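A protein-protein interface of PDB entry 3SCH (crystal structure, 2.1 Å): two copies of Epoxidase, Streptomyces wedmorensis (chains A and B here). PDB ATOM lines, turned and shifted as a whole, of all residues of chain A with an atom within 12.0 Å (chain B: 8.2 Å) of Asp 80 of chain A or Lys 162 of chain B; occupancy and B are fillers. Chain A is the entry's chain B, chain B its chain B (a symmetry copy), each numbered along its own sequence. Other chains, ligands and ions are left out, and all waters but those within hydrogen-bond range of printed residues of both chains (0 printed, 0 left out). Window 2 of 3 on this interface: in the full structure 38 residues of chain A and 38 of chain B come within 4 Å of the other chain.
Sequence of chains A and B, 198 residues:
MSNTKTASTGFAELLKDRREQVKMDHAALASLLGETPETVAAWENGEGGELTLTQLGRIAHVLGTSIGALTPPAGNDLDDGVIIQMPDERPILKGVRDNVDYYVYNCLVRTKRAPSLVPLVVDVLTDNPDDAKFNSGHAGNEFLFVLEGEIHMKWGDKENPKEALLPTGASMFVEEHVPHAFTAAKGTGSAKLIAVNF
Among the printed residues, pairs that only touch across the chains: Leu 78 of chain A with Phe 173 of chain B (3.8 Å), Leu 78 of chain A with Glu 175 of chain B (3.5 Å), Asp 80 of chain A with Trp 155 of chain B (3.5 Å), Asp 80 of chain A with Val 178 of chain B (3.7 Å), Gly 81 of chain A with Phe 173 of chain B (3.9 Å), Gly 81 of chain A with Val 174 of chain B (3.7 Å), Gly 81 of chain A with Val 178 of chain B (3.7 Å), Val 82 of chain A with Trp 155 of chain B (3.3 Å), Val 82 of chain A with Phe 173 of chain B (3.4 Å) and Thr 111 of chain A with Phe 173 of chain B (3.8 Å).
Hydrophobic or aromatic side chains of chain B within 4 Å of the printed part of chain A: Trp 155, Phe 173 and Val 178.
Among the printed residues, 16 pairs touch across the chains.
Among the printed residues, Asp or Glu carboxylates within 4 Å of a Lys or Arg side-chain nitrogen of the other chain: Asp 79 of chain A with Lys 162 of chain B (2.8 Å), Asp 80 of chain A with Lys 162 of chain B (3.6 Å) and Arg 113 of chain A with Glu 175 of chain B (2.7 Å).
NE1 of Trp 155 of chain B lies within hydrogen-bond range of O of Asp 79 of chain A (2.9 Å).
The side-chain carboxylate of Asp 79 of chain A lies within salt-bridge range of the side-chain amino group of Lys 162 of chain B, 2.8 Å away.
The side-chain carboxylate (OD2) of Asp 80 of chain A is in salt-bridge range of the side-chain amino group (NZ) of Lys 162 of chain B, at 3.6 Å.
The backbone carbonyl oxygen (O) of Gly 81 of chain A sits at hydrogen-bond distance from the backbone NH (N) of Glu 175 of chain B, 2.9 Å away.
The backbone carbonyl oxygen (O) of Ile 83 of chain A lies within hydrogen-bond range of the backbone NH (N) of Phe 173 of chain B (2.9 Å).
The side-chain carboxylate (OE1) of Glu 175 of chain B is in salt-bridge range of the guanidinium group (NE) of Arg 113 of chain A, at 2.7 Å.
ND2 of Asn 76 of chain A sits close to N of Leu 78 of chain A, 2.8 Å away.
OD2 of Asp 77 of chain A lies within hydrogen-bond range of OG1 of Thr 111 of chain A.
N of Arg 113 of chain A lies within hydrogen-bond range of OG1 of Thr 111 of chain A (3.0 Å).
N of Lys 162 of chain B is in hydrogen-bond range of O of Trp 155 of chain B (2.8 Å).
O of Val 178 of chain B lies within hydrogen-bond range of ND1 of His 180 of chain B.
Asn 76 of chain A touches none of the printed residues of chain B.
Asp 80 of chain A touches just these residues of chain B: Trp 155 (3.5 Å), Lys 162 (3.5 Å) and Val 178 (3.7 Å).
Printed residues of chain B within 4 Å of Gly 81 of chain A: Phe 173 (3.9 Å), Val 174 (3.7 Å), Glu 175 (2.9 Å) and Val 178 (3.7 Å).
Printed residues of chain B within 4 Å of Val 82 of chain A: Trp 155 (3.3 Å) and Phe 173 (3.4 Å).
Of the printed residues of chain B, Ile 83 of chain A touches Phe 173 (2.9 Å).
No residue of chain A comes within 4 Å of Lys 154 of chain B.
Trp 155 of chain B touches just these residues of chain A: Asp 79, Asp 80 and Val 82.
No residue of chain A comes within 4 Å of Gly 156 of chain B.
Of chain A, only Asp 79 (2.8 Å) and Asp 80 (3.5 Å) come within 4 Å of Lys 162 of chain B.
No residue of chain A comes within 4 Å of Ala 164 of chain B.
Of the printed residues of chain A, Val 174 of chain B touches Gly 81.
The nearest residue of chain B that does not touch Asp 80 of chain A is Gly 156 of chain B (5.1 Å).
No position is printed for both chains.
Of the 16 pairs that touch across the chains among the printed residues, none has its exchanged pair printed and touching as well.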
ATOM      1  N   GLY A  75       1.951   6.714  23.469  1.00  0.00           N
ATOM      2  CA  GLY A  75       2.717   6.161  22.367  1.00  0.00           C
ATOM      3  C   GLY A  75       3.497   4.932  22.793  1.00  0.00           C
ATOM      4  O   GLY A  75       3.574   4.625  23.984  1.00  0.00           O
ATOM      5  N   ASN A  76       4.078   4.229  21.825  1.00  0.00           N
ATOM      6  CA  ASN A  76       4.810   3.002  22.120  1.00  0.00           C
ATOM      7  C   ASN A  76       6.269   3.129  21.737  1.00  0.00           C
ATOM      8  O   ASN A  76       6.611   3.187  20.558  1.00  0.00           O
ATOM      9  CB  ASN A  76       4.161   1.841  21.369  1.00  0.00           C
ATOM     10  CG  ASN A  76       4.647   0.480  21.846  1.00  0.00           C
ATOM     11  OD1 ASN A  76       3.908  -0.507  21.788  1.00  0.00           O
ATOM     12  ND2 ASN A  76       5.884   0.417  22.303  1.00  0.00           N
ATOM     13  N   ASP A  77       7.134   3.173  22.742  1.00  0.00           N
ATOM     14  CA  ASP A  77       8.567   3.303  22.515  1.00  0.00           C
ATOM     15  C   ASP A  77       9.298   2.009  22.843  1.00  0.00           C
ATOM     16  O   ASP A  77      10.480   2.030  23.158  1.00  0.00           O
ATOM     17  CB  ASP A  77       9.115   4.438  23.382  1.00  0.00           C
ATOM     18  CG  ASP A  77       8.678   4.322  24.835  1.00  0.00           C
ATOM     19  OD1 ASP A  77       8.924   5.276  25.608  1.00  0.00           O
ATOM     20  OD2 ASP A  77       8.092   3.284  25.212  1.00  0.00           O
ATOM     21  N   LEU A  78       8.591   0.887  22.777  1.00  0.00           N
ATOM     22  CA  LEU A  78       9.197  -0.397  23.098  1.00  0.00           C
ATOM     23  C   LEU A  78       9.673  -1.174  21.866  1.00  0.00           C
ATOM     24  O   LEU A  78       9.226  -0.931  20.741  1.00  0.00           O
ATOM     25  CB  LEU A  78       8.203  -1.248  23.879  1.00  0.00           C
ATOM     26  CG  LEU A  78       7.610  -0.610  25.138  1.00  0.00           C
ATOM     27  CD1 LEU A  78       6.505  -1.478  25.677  1.00  0.00           C
ATOM     28  CD2 LEU A  78       8.695  -0.427  26.183  1.00  0.00           C
ATOM     29  N   ASP A  79      10.596  -2.103  22.099  1.00  0.00           N
ATOM     30  CA  ASP A  79      11.142  -2.974  21.061  1.00  0.00           C
ATOM     31  C   ASP A  79      10.590  -4.351  21.426  1.00  0.00           C
ATOM     32  O   ASP A  79      11.126  -5.035  22.303  1.00  0.00           O
ATOM     33  CB  ASP A  79      12.676  -2.969  21.121  1.00  0.00           C
ATOM     34  CG  ASP A  79      13.301  -4.014  20.214  1.00  0.00           C
ATOM     35  OD1 ASP A  79      12.579  -4.545  19.347  1.00  0.00           O
ATOM     36  OD2 ASP A  79      14.511  -4.306  20.359  1.00  0.00           O
ATOM     37  N   ASP A  80       9.504  -4.748  20.768  1.00  0.00           N
ATOM     38  CA  ASP A  80       8.850  -6.014  21.063  1.00  0.00           C
ATOM     39  C   ASP A  80       8.487  -6.149  22.537  1.00  0.00           C
ATOM     40  O   ASP A  80       8.635  -7.218  23.132  1.00  0.00           O
ATOM     41  CB  ASP A  80       9.720  -7.195  20.641  1.00  0.00           C
ATOM     42  CG  ASP A  80       9.648  -7.454  19.148  1.00  0.00           C
ATOM     43  OD1 ASP A  80       8.517  -7.483  18.614  1.00  0.00           O
ATOM     44  OD2 ASP A  80      10.710  -7.631  18.515  1.00  0.00           O
ATOM     45  N   GLY A  81       8.027  -5.053  23.129  1.00  0.00           N
ATOM     46  CA  GLY A  81       7.605  -5.097  24.515  1.00  0.00           C
ATOM     47  C   GLY A  81       8.659  -4.754  25.547  1.00  0.00           C
ATOM     48  O   GLY A  81       8.366  -4.775  26.746  1.00  0.00           O
ATOM     49  N   VAL A  82       9.867  -4.416  25.102  1.00  0.00           N
ATOM     50  CA  VAL A  82      10.951  -4.093  26.031  1.00  0.00           C
ATOM     51  C   VAL A  82      11.729  -2.816  25.727  1.00  0.00           C
ATOM     52  O   VAL A  82      11.877  -2.401  24.577  1.00  0.00           O
ATOM     53  CB  VAL A  82      11.981  -5.277  26.087  1.00  0.00           C
ATOM     54  CG1 VAL A  82      13.202  -4.901  26.894  1.00  0.00           C
ATOM     55  CG2 VAL A  82      11.330  -6.502  26.656  1.00  0.00           C
ATOM     56  N   ILE A  83      12.201  -2.158  26.774  1.00  0.00           N
ATOM     57  CA  ILE A  83      13.050  -0.999  26.574  1.00  0.00           C
ATOM     58  C   ILE A  83      14.118  -1.144  27.642  1.00  0.00           C
ATOM     59  O   ILE A  83      13.803  -1.441  28.789  1.00  0.00           O
ATOM     60  CB  ILE A  83      12.303   0.350  26.715  1.00  0.00           C
ATOM     61  CG1 ILE A  83      13.293   1.494  26.503  1.00  0.00           C
ATOM     62  CG2 ILE A  83      11.626   0.465  28.086  1.00  0.00           C
ATOM     63  CD1 ILE A  83      12.642   2.854  26.336  1.00  0.00           C
ATOM     64  N   ILE A  84      15.384  -0.990  27.253  1.00  0.00           N
ATOM     65  CA  ILE A  84      16.480  -1.118  28.200  1.00  0.00           C
ATOM     66  C   ILE A  84      17.285   0.165  28.204  1.00  0.00           C
ATOM     67  O   ILE A  84      17.196   0.969  27.281  1.00  0.00           O
ATOM     68  CB  ILE A  84      17.418  -2.348  27.867  1.00  0.00           C
ATOM     69  CG1 ILE A  84      18.384  -2.022  26.733  1.00  0.00           C
ATOM     70  CG2 ILE A  84      16.586  -3.561  27.412  1.00  0.00           C
ATOM     71  CD1 ILE A  84      19.706  -1.481  27.218  1.00  0.00           C
ATOM     72  N   THR A 111       9.313   4.655  30.134  1.00  0.00           N
ATOM     73  CA  THR A 111       8.590   4.293  28.931  1.00  0.00           C
ATOM     74  C   THR A 111       7.222   4.950  28.853  1.00  0.00           C
ATOM     75  O   THR A 111       6.502   5.028  29.846  1.00  0.00           O
ATOM     76  CB  THR A 111       8.357   2.783  28.862  1.00  0.00           C
ATOM     77  OG1 THR A 111       7.457   2.488  27.788  1.00  0.00           O
ATOM     78  CG2 THR A 111       7.739   2.294  30.172  1.00  0.00           C
ATOM     79  N   ARG A 113       4.776   3.712  27.600  1.00  0.00           N
ATOM     80  CA  ARG A 113       3.751   2.688  27.774  1.00  0.00           C
ATOM     81  C   ARG A 113       3.352   2.568  29.240  1.00  0.00           C
ATOM     82  O   ARG A 113       2.358   1.918  29.561  1.00  0.00           O
ATOM     83  CB  ARG A 113       4.225   1.343  27.232  1.00  0.00           C
ATOM     84  CG  ARG A 113       4.341   1.339  25.713  1.00  0.00           C
ATOM     85  CD  ARG A 113       2.965   1.283  25.039  1.00  0.00           C
ATOM     86  NE  ARG A 113       2.443  -0.078  25.064  1.00  0.00           N
ATOM     87  CZ  ARG A 113       1.318  -0.475  24.481  1.00  0.00           C
ATOM     88  NH1 ARG A 113       0.550   0.384  23.808  1.00  0.00           N
ATOM     89  NH2 ARG A 113       0.972  -1.750  24.560  1.00  0.00           N
ATOM     90  N   PHE B 134      12.583 -19.709  29.128  1.00  0.00           N
ATOM     91  CA  PHE B 134      11.579 -18.661  29.048  1.00  0.00           C
ATOM     92  C   PHE B 134      10.358 -18.905  29.911  1.00  0.00           C
ATOM     93  O   PHE B 134       9.938 -20.046  30.107  1.00  0.00           O
ATOM     94  CB  PHE B 134      11.060 -18.523  27.613  1.00  0.00           C
ATOM     95  CG  PHE B 134      11.955 -17.748  26.702  1.00  0.00           C
ATOM     96  CD1 PHE B 134      13.129 -18.307  26.211  1.00  0.00           C
ATOM     97  CD2 PHE B 134      11.615 -16.452  26.323  1.00  0.00           C
ATOM     98  CE1 PHE B 134      13.951 -17.585  25.350  1.00  0.00           C
ATOM     99  CE2 PHE B 134      12.430 -15.721  25.462  1.00  0.00           C
ATOM    100  CZ  PHE B 134      13.601 -16.292  24.974  1.00  0.00           C
ATOM    101  N   HIS B 152      22.392 -11.623  30.645  1.00  0.00           N
ATOM    102  CA  HIS B 152      22.141 -11.887  29.230  1.00  0.00           C
ATOM    103  C   HIS B 152      20.634 -12.114  29.207  1.00  0.00           C
ATOM    104  O   HIS B 152      20.162 -13.136  29.679  1.00  0.00           O
ATOM    105  CB  HIS B 152      22.865 -13.163  28.772  1.00  0.00           C
ATOM    106  CG  HIS B 152      22.724 -13.443  27.305  1.00  0.00           C
ATOM    107  ND1 HIS B 152      23.804 -13.706  26.490  1.00  0.00           N
ATOM    108  CD2 HIS B 152      21.632 -13.466  26.502  1.00  0.00           C
ATOM    109  CE1 HIS B 152      23.384 -13.871  25.248  1.00  0.00           C
ATOM    110  NE2 HIS B 152      22.071 -13.730  25.227  1.00  0.00           N
ATOM    111  N   MET B 153      19.883 -11.154  28.674  1.00  0.00           N
ATOM    112  CA  MET B 153      18.429 -11.257  28.634  1.00  0.00           C
ATOM    113  C   MET B 153      17.913 -11.663  27.268  1.00  0.00           C
ATOM    114  O   MET B 153      18.518 -11.327  26.261  1.00  0.00           O
ATOM    115  CB  MET B 153      17.834  -9.902  29.033  1.00  0.00           C
ATOM    116  CG  MET B 153      16.389  -9.643  28.627  1.00  0.00           C
ATOM    117  SD  MET B 153      15.874  -7.817  29.154  1.00  0.00           S
ATOM    118  CE  MET B 153      14.002  -8.094  29.493  1.00  0.00           C
ATOM    119  N   LYS B 154      16.800 -12.391  27.239  1.00  0.00           N
ATOM    120  CA  LYS B 154      16.174 -12.788  25.976  1.00  0.00           C
ATOM    121  C   LYS B 154      14.678 -12.531  26.078  1.00  0.00           C
ATOM    122  O   LYS B 154      14.069 -12.789  27.119  1.00  0.00           O
ATOM    123  CB  LYS B 154      16.406 -14.269  25.680  1.00  0.00           C
ATOM    124  CG  LYS B 154      17.857 -14.649  25.452  1.00  0.00           C
ATOM    125  CD  LYS B 154      17.926 -16.053  24.875  1.00  0.00           C
ATOM    126  CE  LYS B 154      19.322 -16.640  24.978  1.00  0.00           C
ATOM    127  NZ  LYS B 154      19.372 -18.000  24.355  1.00  0.00           N
ATOM    128  N   TRP B 155      14.071 -12.030  25.013  1.00  0.00           N
ATOM    129  CA  TRP B 155      12.642 -11.789  25.095  1.00  0.00           C
ATOM    130  C   TRP B 155      11.944 -11.931  23.765  1.00  0.00           C
ATOM    131  O   TRP B 155      12.588 -12.002  22.724  1.00  0.00           O
ATOM    132  CB  TRP B 155      12.367 -10.408  25.711  1.00  0.00           C
ATOM    133  CG  TRP B 155      12.617  -9.209  24.832  1.00  0.00           C
ATOM    134  CD1 TRP B 155      11.703  -8.562  24.055  1.00  0.00           C
ATOM    135  CD2 TRP B 155      13.838  -8.465  24.717  1.00  0.00           C
ATOM    136  NE1 TRP B 155      12.274  -7.451  23.474  1.00  0.00           N
ATOM    137  CE2 TRP B 155      13.583  -7.370  23.864  1.00  0.00           C
ATOM    138  CE3 TRP B 155      15.123  -8.618  25.254  1.00  0.00           C
ATOM    139  CZ2 TRP B 155      14.560  -6.427  23.539  1.00  0.00           C
ATOM    140  CZ3 TRP B 155      16.097  -7.684  24.929  1.00  0.00           C
ATOM    141  CH2 TRP B 155      15.807  -6.598  24.077  1.00  0.00           C
ATOM    142  N   GLY B 156      10.620 -11.986  23.814  1.00  0.00           N
ATOM    143  CA  GLY B 156       9.844 -12.113  22.597  1.00  0.00           C
ATOM    144  C   GLY B 156       9.682 -13.559  22.166  1.00  0.00           C
ATOM    145  O   GLY B 156       9.447 -14.442  22.993  1.00  0.00           O
ATOM    146  N   ASP B 157       9.802 -13.804  20.866  1.00  0.00           N
ATOM    147  CA  ASP B 157       9.666 -15.154  20.321  1.00  0.00           C
ATOM    148  C   ASP B 157      10.860 -15.992  20.770  1.00  0.00           C
ATOM    149  O   ASP B 157      11.972 -15.792  20.291  1.00  0.00           O
ATOM    150  CB  ASP B 157       9.628 -15.089  18.789  1.00  0.00           C
ATOM    151  CG  ASP B 157       9.467 -16.461  18.148  1.00  0.00           C
ATOM    152  OD1 ASP B 157       9.586 -16.549  16.905  1.00  0.00           O
ATOM    153  OD2 ASP B 157       9.221 -17.441  18.883  1.00  0.00           O
ATOM    154  N   LYS B 158      10.637 -16.940  21.675  1.00  0.00           N
ATOM    155  CA  LYS B 158      11.749 -17.751  22.161  1.00  0.00           C
ATOM    156  C   LYS B 158      12.498 -18.540  21.084  1.00  0.00           C
ATOM    157  O   LYS B 158      13.606 -19.023  21.323  1.00  0.00           O
ATOM    158  CB  LYS B 158      11.286 -18.694  23.278  1.00  0.00           C
ATOM    159  CG  LYS B 158      10.528 -19.922  22.828  1.00  0.00           C
ATOM    160  CD  LYS B 158      10.349 -20.869  24.007  1.00  0.00           C
ATOM    161  CE  LYS B 158       9.795 -22.217  23.581  1.00  0.00           C
ATOM    162  NZ  LYS B 158       8.437 -22.085  23.006  1.00  0.00           N
ATOM    163  N   GLU B 159      11.912 -18.663  19.897  1.00  0.00           N
ATOM    164  CA  GLU B 159      12.575 -19.386  18.814  1.00  0.00           C
ATOM    165  C   GLU B 159      13.502 -18.466  18.018  1.00  0.00           C
ATOM    166  O   GLU B 159      14.413 -18.933  17.330  1.00  0.00           O
ATOM    167  CB  GLU B 159      11.540 -20.020  17.875  1.00  0.00           C
ATOM    168  CG  GLU B 159      10.778 -21.199  18.491  1.00  0.00           C
ATOM    169  CD  GLU B 159      11.701 -22.318  18.962  1.00  0.00           C
ATOM    170  OE1 GLU B 159      12.520 -22.803  18.143  1.00  0.00           O
ATOM    171  OE2 GLU B 159      11.610 -22.721  20.149  1.00  0.00           O
ATOM    172  N   ASN B 160      13.267 -17.161  18.131  1.00  0.00           N
ATOM    173  CA  ASN B 160      14.049 -16.133  17.442  1.00  0.00           C
ATOM    174  C   ASN B 160      13.863 -14.872  18.294  1.00  0.00           C
ATOM    175  O   ASN B 160      13.271 -13.886  17.853  1.00  0.00           O
ATOM    176  CB  ASN B 160      13.482 -15.937  16.035  1.00  0.00           C
ATOM    177  CG  ASN B 160      14.200 -14.859  15.248  1.00  0.00           C
ATOM    178  OD1 ASN B 160      15.429 -14.838  15.168  1.00  0.00           O
ATOM    179  ND2 ASN B 160      13.427 -13.963  14.642  1.00  0.00           N
ATOM    180  N   PRO B 161      14.379 -14.895  19.535  1.00  0.00           N
ATOM    181  CA  PRO B 161      14.277 -13.791  20.490  1.00  0.00           C
ATOM    182  C   PRO B 161      15.158 -12.579  20.297  1.00  0.00           C
ATOM    183  O   PRO B 161      16.161 -12.617  19.595  1.00  0.00           O
ATOM    184  CB  PRO B 161      14.585 -14.473  21.818  1.00  0.00           C
ATOM    185  CG  PRO B 161      15.669 -15.416  21.422  1.00  0.00           C
ATOM    186  CD  PRO B 161      15.112 -16.024  20.137  1.00  0.00           C
ATOM    187  N   LYS B 162      14.744 -11.495  20.940  1.00  0.00           N
ATOM    188  CA  LYS B 162      15.506 -10.265  20.943  1.00  0.00           C
ATOM    189  C   LYS B 162      16.410 -10.529  22.144  1.00  0.00           C
ATOM    190  O   LYS B 162      16.019 -11.259  23.056  1.00  0.00           O
ATOM    191  CB  LYS B 162      14.598  -9.065  21.213  1.00  0.00           C
ATOM    192  CG  LYS B 162      13.510  -8.858  20.165  1.00  0.00           C
ATOM    193  CD  LYS B 162      14.097  -8.812  18.772  1.00  0.00           C
ATOM    194  CE  LYS B 162      14.946  -7.579  18.539  1.00  0.00           C
ATOM    195  NZ  LYS B 162      14.093  -6.460  18.042  1.00  0.00           N
ATOM    196  N   GLU B 163      17.612  -9.965  22.144  1.00  0.00           N
ATOM    197  CA  GLU B 163      18.535 -10.198  23.244  1.00  0.00           C
ATOM    198  C   GLU B 163      19.320  -8.955  23.605  1.00  0.00           C
ATOM    199  O   GLU B 163      19.441  -8.023  22.799  1.00  0.00           O
ATOM    200  CB  GLU B 163      19.547 -11.278  22.868  1.00  0.00           C
ATOM    201  CG  GLU B 163      18.986 -12.546  22.255  1.00  0.00           C
ATOM    202  CD  GLU B 163      20.101 -13.498  21.852  1.00  0.00           C
ATOM    203  OE1 GLU B 163      20.665 -14.178  22.737  1.00  0.00           O
ATOM    204  OE2 GLU B 163      20.437 -13.547  20.648  1.00  0.00           O
ATOM    205  N   ALA B 164      19.868  -8.949  24.818  1.00  0.00           N
ATOM    206  CA  ALA B 164      20.682  -7.839  25.269  1.00  0.00           C
ATOM    207  C   ALA B 164      21.644  -8.275  26.362  1.00  0.00           C
ATOM    208  O   ALA B 164      21.286  -9.069  27.231  1.00  0.00           O
ATOM    209  CB  ALA B 164      19.797  -6.705  25.772  1.00  0.00           C
ATOM    210  N   LEU B 165      22.874  -7.774  26.298  1.00  0.00           N
ATOM    211  CA  LEU B 165      23.886  -8.061  27.314  1.00  0.00           C
ATOM    212  C   LEU B 165      23.775  -6.836  28.195  1.00  0.00           C
ATOM    213  O   LEU B 165      23.933  -5.722  27.723  1.00  0.00           O
ATOM    214  CB  LEU B 165      25.289  -8.143  26.697  1.00  0.00           C
ATOM    215  CG  LEU B 165      25.706  -9.545  26.245  1.00  0.00           C
ATOM    216  CD1 LEU B 165      25.781 -10.484  27.434  1.00  0.00           C
ATOM    217  CD2 LEU B 165      24.690 -10.076  25.273  1.00  0.00           C
ATOM    218  N   PHE B 173      12.622  -2.434  31.235  1.00  0.00           N
ATOM    219  CA  PHE B 173      11.191  -2.468  31.455  1.00  0.00           C
ATOM    220  C   PHE B 173      10.653  -3.554  30.539  1.00  0.00           C
ATOM    221  O   PHE B 173      10.989  -3.592  29.350  1.00  0.00           O
ATOM    222  CB  PHE B 173      10.544  -1.125  31.101  1.00  0.00           C
ATOM    223  CG  PHE B 173       9.040  -1.184  31.034  1.00  0.00           C
ATOM    224  CD1 PHE B 173       8.267  -0.972  32.169  1.00  0.00           C
ATOM    225  CD2 PHE B 173       8.397  -1.490  29.834  1.00  0.00           C
ATOM    226  CE1 PHE B 173       6.874  -1.067  32.113  1.00  0.00           C
ATOM    227  CE2 PHE B 173       7.009  -1.584  29.771  1.00  0.00           C
ATOM    228  CZ  PHE B 173       6.247  -1.372  30.914  1.00  0.00           C
ATOM    229  N   VAL B 174       9.840  -4.446  31.090  1.00  0.00           N
ATOM    230  CA  VAL B 174       9.243  -5.523  30.310  1.00  0.00           C
ATOM    231  C   VAL B 174       7.726  -5.412  30.451  1.00  0.00           C
ATOM    232  O   VAL B 174       7.191  -5.521  31.553  1.00  0.00           O
ATOM    233  CB  VAL B 174       9.688  -6.932  30.815  1.00  0.00           C
ATOM    234  CG1 VAL B 174       9.109  -8.011  29.905  1.00  0.00           C
ATOM    235  CG2 VAL B 174      11.209  -7.025  30.859  1.00  0.00           C
ATOM    236  N   GLU B 175       7.047  -5.203  29.327  1.00  0.00           N
ATOM    237  CA  GLU B 175       5.590  -5.049  29.300  1.00  0.00           C
ATOM    238  C   GLU B 175       4.844  -6.335  29.640  1.00  0.00           C
ATOM    239  O   GLU B 175       5.362  -7.437  29.455  1.00  0.00           O
ATOM    240  CB  GLU B 175       5.160  -4.555  27.918  1.00  0.00           C
ATOM    241  CG  GLU B 175       3.742  -4.067  27.847  1.00  0.00           C
ATOM    242  CD  GLU B 175       3.466  -3.334  26.545  1.00  0.00           C
ATOM    243  OE1 GLU B 175       2.844  -2.257  26.602  1.00  0.00           O
ATOM    244  OE2 GLU B 175       3.875  -3.835  25.474  1.00  0.00           O
ATOM    245  N   HIS B 177       2.790  -9.595  29.679  1.00  0.00           N
ATOM    246  CA  HIS B 177       2.541 -10.618  28.672  1.00  0.00           C
ATOM    247  C   HIS B 177       3.701 -10.833  27.698  1.00  0.00           C
ATOM    248  O   HIS B 177       3.563 -11.594  26.740  1.00  0.00           O
ATOM    249  CB  HIS B 177       1.262 -10.295  27.893  1.00  0.00           C
ATOM    250  CG  HIS B 177       0.028 -10.282  28.739  1.00  0.00           C
ATOM    251  ND1 HIS B 177      -0.215 -11.223  29.717  1.00  0.00           N
ATOM    252  CD2 HIS B 177      -1.035  -9.443  28.754  1.00  0.00           C
ATOM    253  CE1 HIS B 177      -1.373 -10.964  30.296  1.00  0.00           C
ATOM    254  NE2 HIS B 177      -1.892  -9.890  29.731  1.00  0.00           N
ATOM    255  N   VAL B 178       4.840 -10.182  27.926  1.00  0.00           N
ATOM    256  CA  VAL B 178       5.983 -10.402  27.035  1.00  0.00           C
ATOM    257  C   VAL B 178       6.870 -11.526  27.595  1.00  0.00           C
ATOM    258  O   VAL B 178       7.389 -11.407  28.700  1.00  0.00           O
ATOM    259  CB  VAL B 178       6.856  -9.126  26.910  1.00  0.00           C
ATOM    260  CG1 VAL B 178       8.081  -9.418  26.069  1.00  0.00           C
ATOM    261  CG2 VAL B 178       6.046  -7.991  26.296  1.00  0.00           C
ATOM    262  N   PRO B 179       7.042 -12.638  26.853  1.00  0.00           N
ATOM    263  CA  PRO B 179       7.891 -13.720  27.370  1.00  0.00           C
ATOM    264  C   PRO B 179       9.349 -13.296  27.490  1.00  0.00           C
ATOM    265  O   PRO B 179       9.866 -12.573  26.633  1.00  0.00           O
ATOM    266  CB  PRO B 179       7.690 -14.848  26.347  1.00  0.00           C
ATOM    267  CG  PRO B 179       7.320 -14.121  25.102  1.00  0.00           C
ATOM    268  CD  PRO B 179       6.412 -13.036  25.582  1.00  0.00           C
ATOM    269  N   HIS B 180      10.010 -13.729  28.559  1.00  0.00           N
ATOM    270  CA  HIS B 180      11.412 -13.377  28.761  1.00  0.00           C
ATOM    271  C   HIS B 180      12.176 -14.403  29.597  1.00  0.00           C
ATOM    272  O   HIS B 180      11.581 -15.211  30.314  1.00  0.00           O
ATOM    273  CB  HIS B 180      11.521 -12.004  29.416  1.00  0.00           C
ATOM    274  CG  HIS B 180      10.594 -11.820  30.569  1.00  0.00           C
ATOM    275  ND1 HIS B 180       9.225 -11.728  30.437  1.00  0.00           N
ATOM    276  CD2 HIS B 180      10.850 -11.695  31.897  1.00  0.00           C
ATOM    277  CE1 HIS B 180       8.698 -11.550  31.646  1.00  0.00           C
ATOM    278  NE2 HIS B 180       9.642 -11.521  32.560  1.00  0.00           N
ATOM    279  N   ALA B 181      13.500 -14.336  29.503  1.00  0.00           N
ATOM    280  CA  ALA B 181      14.402 -15.245  30.206  1.00  0.00           C
ATOM    281  C   ALA B 181      15.721 -14.542  30.498  1.00  0.00           C
ATOM    282  O   ALA B 181      16.126 -13.631  29.774  1.00  0.00           O
ATOM    283  CB  ALA B 181      14.653 -16.473  29.351  1.00  0.00           C
